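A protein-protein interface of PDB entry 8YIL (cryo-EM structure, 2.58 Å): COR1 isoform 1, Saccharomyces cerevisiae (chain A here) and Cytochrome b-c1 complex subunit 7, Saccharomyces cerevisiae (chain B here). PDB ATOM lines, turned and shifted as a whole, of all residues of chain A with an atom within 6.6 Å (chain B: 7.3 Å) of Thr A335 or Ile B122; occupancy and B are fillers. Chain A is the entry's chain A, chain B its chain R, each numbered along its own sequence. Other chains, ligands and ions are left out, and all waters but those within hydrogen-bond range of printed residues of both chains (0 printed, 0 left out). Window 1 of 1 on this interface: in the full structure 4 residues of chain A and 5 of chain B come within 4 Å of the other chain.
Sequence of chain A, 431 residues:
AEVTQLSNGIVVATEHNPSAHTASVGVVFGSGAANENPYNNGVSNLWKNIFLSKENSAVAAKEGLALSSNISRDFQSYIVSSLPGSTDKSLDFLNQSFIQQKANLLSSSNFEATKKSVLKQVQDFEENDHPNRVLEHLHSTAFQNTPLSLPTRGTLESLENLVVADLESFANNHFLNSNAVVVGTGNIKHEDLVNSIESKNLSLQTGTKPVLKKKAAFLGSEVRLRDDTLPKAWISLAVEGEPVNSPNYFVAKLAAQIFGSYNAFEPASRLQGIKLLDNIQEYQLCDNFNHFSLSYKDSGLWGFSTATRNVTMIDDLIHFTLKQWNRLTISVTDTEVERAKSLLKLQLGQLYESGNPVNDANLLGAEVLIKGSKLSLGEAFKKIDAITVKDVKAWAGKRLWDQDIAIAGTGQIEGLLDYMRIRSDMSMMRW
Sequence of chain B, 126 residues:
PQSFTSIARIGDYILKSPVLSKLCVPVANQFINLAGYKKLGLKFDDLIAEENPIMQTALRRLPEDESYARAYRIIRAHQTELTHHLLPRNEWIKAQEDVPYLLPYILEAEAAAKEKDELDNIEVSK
The side-chain amino group (NZ) of Lys A275 is in salt-bridge range of the side-chain carboxylate (OE2) of Glu A336, at 3.99 Å.
Among the printed residues, pairs that only touch across the chains: Thr A335 with Val B124 (3.6 Å), Thr A335 with Ile B122 (3.6 Å), Lys A275 with Asp B120 (3.9 Å) and Asp A334 with Ser B125 (3.99 Å).
Of the printed residues of chain B, Thr A335 touches Ile B122 and Val B124. Of chain A, only Thr A335 comes within 4 Å of Ile B122. Printed residues of chain B within 4 Å of Lys A275: Asp B120 (3.9 Å). Of the printed residues of chain A, Val B124 touches Thr A335 (3.6 Å). Printed residues of chain B within 4 Å of Asp A334: Ser B125 (3.99 Å). Of the printed residues of chain A, Asp B120 touches Lys A275. Glu B118 touches none of the printed residues of chain A. Leu B119 touches none of the printed residues of chain A. The nearest residue of chain B that does not touch Thr A335 is Glu B123 (5.1 Å). The nearest residue of chain A that does not touch Ile B122 is Thr A333 (5.9 Å). The nearest printed residue of chain A that does not touch Asp B120 is Thr A335 (5.8 Å).
Hydrophobic or aromatic side chains of chain B within 4 Å of the printed part of chain A: Ile B122 and Val B124. Printed residues of chain A that touch a printed residue of chain B: Lys A275, Asp A334 and Thr A335. Among the printed residues, 4 pairs touch across the chains. Among the printed residues, no Asp or Glu carboxylate lies within 4 Å of a Lys or Arg side-chain nitrogen of the other chain.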
ATOM      1  N   LYS A 275     -20.635  27.212 -25.848  1.00  0.00           N
ATOM      2  CA  LYS A 275     -20.430  28.627 -25.558  1.00  0.00           C
ATOM      3  C   LYS A 275     -20.828  29.530 -26.715  1.00  0.00           C
ATOM      4  O   LYS A 275     -21.036  30.727 -26.503  1.00  0.00           O
ATOM      5  CB  LYS A 275     -18.972  28.880 -25.191  1.00  0.00           C
ATOM      6  CG  LYS A 275     -18.592  28.388 -23.816  1.00  0.00           C
ATOM      7  CD  LYS A 275     -17.123  28.628 -23.546  1.00  0.00           C
ATOM      8  CE  LYS A 275     -16.810  28.545 -22.068  1.00  0.00           C
ATOM      9  NZ  LYS A 275     -17.101  27.199 -21.516  1.00  0.00           N
ATOM     10  N   THR A 333     -10.907  24.588 -22.615  1.00  0.00           N
ATOM     11  CA  THR A 333     -10.971  24.174 -21.221  1.00  0.00           C
ATOM     12  C   THR A 333     -11.155  22.665 -21.109  1.00  0.00           C
ATOM     13  O   THR A 333     -11.510  21.980 -22.067  1.00  0.00           O
ATOM     14  CB  THR A 333     -12.101  24.905 -20.499  1.00  0.00           C
ATOM     15  OG1 THR A 333     -13.357  24.428 -20.982  1.00  0.00           O
ATOM     16  CG2 THR A 333     -12.016  26.386 -20.775  1.00  0.00           C
ATOM     17  N   ASP A 334     -10.911  22.153 -19.907  1.00  0.00           N
ATOM     18  CA  ASP A 334     -10.921  20.715 -19.683  1.00  0.00           C
ATOM     19  C   ASP A 334     -12.333  20.160 -19.539  1.00  0.00           C
ATOM     20  O   ASP A 334     -12.550  18.976 -19.809  1.00  0.00           O
ATOM     21  CB  ASP A 334     -10.096  20.387 -18.438  1.00  0.00           C
ATOM     22  CG  ASP A 334      -9.779  18.909 -18.304  1.00  0.00           C
ATOM     23  OD1 ASP A 334      -9.919  18.151 -19.282  1.00  0.00           O
ATOM     24  OD2 ASP A 334      -9.390  18.497 -17.194  1.00  0.00           O
ATOM     25  N   THR A 335     -13.306  20.976 -19.144  1.00  0.00           N
ATOM     26  CA  THR A 335     -14.675  20.481 -19.089  1.00  0.00           C
ATOM     27  C   THR A 335     -15.325  20.411 -20.463  1.00  0.00           C
ATOM     28  O   THR A 335     -16.331  19.717 -20.620  1.00  0.00           O
ATOM     29  CB  THR A 335     -15.533  21.341 -18.160  1.00  0.00           C
ATOM     30  OG1 THR A 335     -16.865  20.818 -18.122  1.00  0.00           O
ATOM     31  CG2 THR A 335     -15.583  22.768 -18.645  1.00  0.00           C
ATOM     32  N   GLU A 336     -14.780  21.108 -21.459  1.00  0.00           N
ATOM     33  CA  GLU A 336     -15.280  20.972 -22.816  1.00  0.00           C
ATOM     34  C   GLU A 336     -14.711  19.753 -23.519  1.00  0.00           C
ATOM     35  O   GLU A 336     -15.347  19.233 -24.438  1.00  0.00           O
ATOM     36  CB  GLU A 336     -14.966  22.232 -23.620  1.00  0.00           C
ATOM     37  CG  GLU A 336     -15.682  23.462 -23.111  1.00  0.00           C
ATOM     38  CD  GLU A 336     -15.578  24.640 -24.053  1.00  0.00           C
ATOM     39  OE1 GLU A 336     -16.510  24.853 -24.855  1.00  0.00           O
ATOM     40  OE2 GLU A 336     -14.564  25.358 -23.990  1.00  0.00           O
ATOM     41  N   VAL A 337     -13.538  19.287 -23.104  1.00  0.00           N
ATOM     42  CA  VAL A 337     -12.965  18.084 -23.691  1.00  0.00           C
ATOM     43  C   VAL A 337     -13.652  16.842 -23.138  1.00  0.00           C
ATOM     44  O   VAL A 337     -13.912  15.884 -23.871  1.00  0.00           O
ATOM     45  CB  VAL A 337     -11.442  18.082 -23.456  1.00  0.00           C
ATOM     46  CG1 VAL A 337     -10.811  16.750 -23.791  1.00  0.00           C
ATOM     47  CG2 VAL A 337     -10.797  19.175 -24.282  1.00  0.00           C
ATOM     48  N   GLU A 338     -14.024  16.861 -21.858  1.00  0.00           N
ATOM     49  CA  GLU A 338     -14.675  15.706 -21.252  1.00  0.00           C
ATOM     50  C   GLU A 338     -16.135  15.578 -21.658  1.00  0.00           C
ATOM     51  O   GLU A 338     -16.672  14.467 -21.657  1.00  0.00           O
ATOM     52  CB  GLU A 338     -14.568  15.779 -19.731  1.00  0.00           C
ATOM     53  CG  GLU A 338     -13.147  15.692 -19.202  1.00  0.00           C
ATOM     54  CD  GLU A 338     -12.506  14.342 -19.453  1.00  0.00           C
ATOM     55  OE1 GLU A 338     -13.172  13.313 -19.221  1.00  0.00           O
ATOM     56  OE2 GLU A 338     -11.337  14.309 -19.884  1.00  0.00           O
ATOM     57  N   ARG A 339     -16.796  16.689 -21.989  1.00  0.00           N
ATOM     58  CA  ARG A 339     -18.170  16.619 -22.476  1.00  0.00           C
ATOM     59  C   ARG A 339     -18.226  16.025 -23.873  1.00  0.00           C
ATOM     60  O   ARG A 339     -19.099  15.206 -24.172  1.00  0.00           O
ATOM     61  CB  ARG A 339     -18.802  18.006 -22.460  1.00  0.00           C
ATOM     62  CG  ARG A 339     -20.174  18.085 -23.087  1.00  0.00           C
ATOM     63  CD  ARG A 339     -20.446  19.464 -23.647  1.00  0.00           C
ATOM     64  NE  ARG A 339     -21.759  19.554 -24.275  1.00  0.00           N
ATOM     65  CZ  ARG A 339     -21.965  19.624 -25.585  1.00  0.00           C
ATOM     66  NH1 ARG A 339     -23.196  19.702 -26.053  1.00  0.00           N
ATOM     67  NH2 ARG A 339     -20.944  19.622 -26.425  1.00  0.00           N
ATOM     68  N   ALA A 340     -17.285  16.409 -24.736  1.00  0.00           N
ATOM     69  CA  ALA A 340     -17.262  15.903 -26.099  1.00  0.00           C
ATOM     70  C   ALA A 340     -16.767  14.468 -26.189  1.00  0.00           C
ATOM     71  O   ALA A 340     -16.985  13.823 -27.215  1.00  0.00           O
ATOM     72  CB  ALA A 340     -16.398  16.802 -26.971  1.00  0.00           C
ATOM     73  N   ASP B 117     -24.971  30.369 -14.525  1.00  0.00           N
ATOM     74  CA  ASP B 117     -23.640  30.952 -14.569  1.00  0.00           C
ATOM     75  C   ASP B 117     -22.611  30.083 -13.856  1.00  0.00           C
ATOM     76  O   ASP B 117     -21.431  30.108 -14.216  1.00  0.00           O
ATOM     77  CB  ASP B 117     -23.676  32.353 -13.963  1.00  0.00           C
ATOM     78  CG  ASP B 117     -22.370  33.089 -14.122  1.00  0.00           C
ATOM     79  OD1 ASP B 117     -22.176  33.751 -15.161  1.00  0.00           O
ATOM     80  OD2 ASP B 117     -21.526  33.006 -13.210  1.00  0.00           O
ATOM     81  N   GLU B 118     -23.021  29.302 -12.861  1.00  0.00           N
ATOM     82  CA  GLU B 118     -22.093  28.395 -12.204  1.00  0.00           C
ATOM     83  C   GLU B 118     -22.003  27.044 -12.890  1.00  0.00           C
ATOM     84  O   GLU B 118     -21.266  26.184 -12.415  1.00  0.00           O
ATOM     85  CB  GLU B 118     -22.472  28.215 -10.732  1.00  0.00           C
ATOM     86  CG  GLU B 118     -23.798  27.541 -10.485  1.00  0.00           C
ATOM     87  CD  GLU B 118     -23.655  26.083 -10.135  1.00  0.00           C
ATOM     88  OE1 GLU B 118     -22.540  25.672  -9.759  1.00  0.00           O
ATOM     89  OE2 GLU B 118     -24.654  25.342 -10.234  1.00  0.00           O
ATOM     90  N   LEU B 119     -22.742  26.829 -13.978  1.00  0.00           N
ATOM     91  CA  LEU B 119     -22.540  25.677 -14.846  1.00  0.00           C
ATOM     92  C   LEU B 119     -21.756  26.022 -16.102  1.00  0.00           C
ATOM     93  O   LEU B 119     -21.401  25.116 -16.858  1.00  0.00           O
ATOM     94  CB  LEU B 119     -23.879  25.054 -15.251  1.00  0.00           C
ATOM     95  CG  LEU B 119     -24.583  24.071 -14.316  1.00  0.00           C
ATOM     96  CD1 LEU B 119     -26.010  23.859 -14.765  1.00  0.00           C
ATOM     97  CD2 LEU B 119     -23.857  22.756 -14.269  1.00  0.00           C
ATOM     98  N   ASP B 120     -21.500  27.301 -16.356  1.00  0.00           N
ATOM     99  CA  ASP B 120     -20.599  27.696 -17.426  1.00  0.00           C
ATOM    100  C   ASP B 120     -19.158  27.789 -16.962  1.00  0.00           C
ATOM    101  O   ASP B 120     -18.251  27.818 -17.799  1.00  0.00           O
ATOM    102  CB  ASP B 120     -21.011  29.044 -18.017  1.00  0.00           C
ATOM    103  CG  ASP B 120     -22.220  28.942 -18.914  1.00  0.00           C
ATOM    104  OD1 ASP B 120     -22.168  28.197 -19.912  1.00  0.00           O
ATOM    105  OD2 ASP B 120     -23.222  29.626 -18.637  1.00  0.00           O
ATOM    106  N   ASN B 121     -18.933  27.843 -15.656  1.00  0.00           N
ATOM    107  CA  ASN B 121     -17.606  27.905 -15.056  1.00  0.00           C
ATOM    108  C   ASN B 121     -17.479  26.645 -14.208  1.00  0.00           C
ATOM    109  O   ASN B 121     -17.918  26.608 -13.060  1.00  0.00           O
ATOM    110  CB  ASN B 121     -17.458  29.161 -14.252  1.00  0.00           C
ATOM    111  CG  ASN B 121     -17.654  30.400 -15.088  1.00  0.00           C
ATOM    112  OD1 ASN B 121     -17.124  30.506 -16.188  1.00  0.00           O
ATOM    113  ND2 ASN B 121     -18.437  31.336 -14.583  1.00  0.00           N
ATOM    114  N   ILE B 122     -16.916  25.600 -14.807  1.00  0.00           N
ATOM    115  CA  ILE B 122     -16.913  24.249 -14.264  1.00  0.00           C
ATOM    116  C   ILE B 122     -15.487  23.706 -14.349  1.00  0.00           C
ATOM    117  O   ILE B 122     -14.767  23.942 -15.317  1.00  0.00           O
ATOM    118  CB  ILE B 122     -17.929  23.346 -15.014  1.00  0.00           C
ATOM    119  CG1 ILE B 122     -19.359  23.725 -14.643  1.00  0.00           C
ATOM    120  CG2 ILE B 122     -17.766  21.869 -14.735  1.00  0.00           C
ATOM    121  CD1 ILE B 122     -19.692  23.441 -13.188  1.00  0.00           C
ATOM    122  N   GLU B 123     -15.087  22.961 -13.317  1.00  0.00           N
ATOM    123  CA  GLU B 123     -13.798  22.281 -13.258  1.00  0.00           C
ATOM    124  C   GLU B 123     -13.973  20.801 -12.946  1.00  0.00           C
ATOM    125  O   GLU B 123     -13.329  20.263 -12.041  1.00  0.00           O
ATOM    126  CB  GLU B 123     -12.871  22.926 -12.232  1.00  0.00           C
ATOM    127  CG  GLU B 123     -12.438  24.323 -12.580  1.00  0.00           C
ATOM    128  CD  GLU B 123     -11.022  24.353 -13.110  1.00  0.00           C
ATOM    129  OE1 GLU B 123     -10.453  25.450 -13.268  1.00  0.00           O
ATOM    130  OE2 GLU B 123     -10.470  23.265 -13.369  1.00  0.00           O
ATOM    131  N   VAL B 124     -14.853  20.113 -13.673  1.00  0.00           N
ATOM    132  CA  VAL B 124     -14.948  18.661 -13.520  1.00  0.00           C
ATOM    133  C   VAL B 124     -13.780  18.038 -14.285  1.00  0.00           C
ATOM    134  O   VAL B 124     -13.484  18.390 -15.431  1.00  0.00           O
ATOM    135  CB  VAL B 124     -16.307  18.096 -13.960  1.00  0.00           C
ATOM    136  CG1 VAL B 124     -17.416  18.581 -13.032  1.00  0.00           C
ATOM    137  CG2 VAL B 124     -16.660  18.414 -15.421  1.00  0.00           C
ATOM    138  N   SER B 125     -13.043  17.182 -13.597  1.00  0.00           N
ATOM    139  CA  SER B 125     -11.997  16.363 -14.179  1.00  0.00           C
ATOM    140  C   SER B 125     -12.511  14.932 -14.309  1.00  0.00           C
ATOM    141  O   SER B 125     -13.700  14.658 -14.125  1.00  0.00           O
ATOM    142  CB  SER B 125     -10.724  16.459 -13.334  1.00  0.00           C
ATOM    143  OG  SER B 125     -10.199  17.775 -13.356  1.00  0.00           O
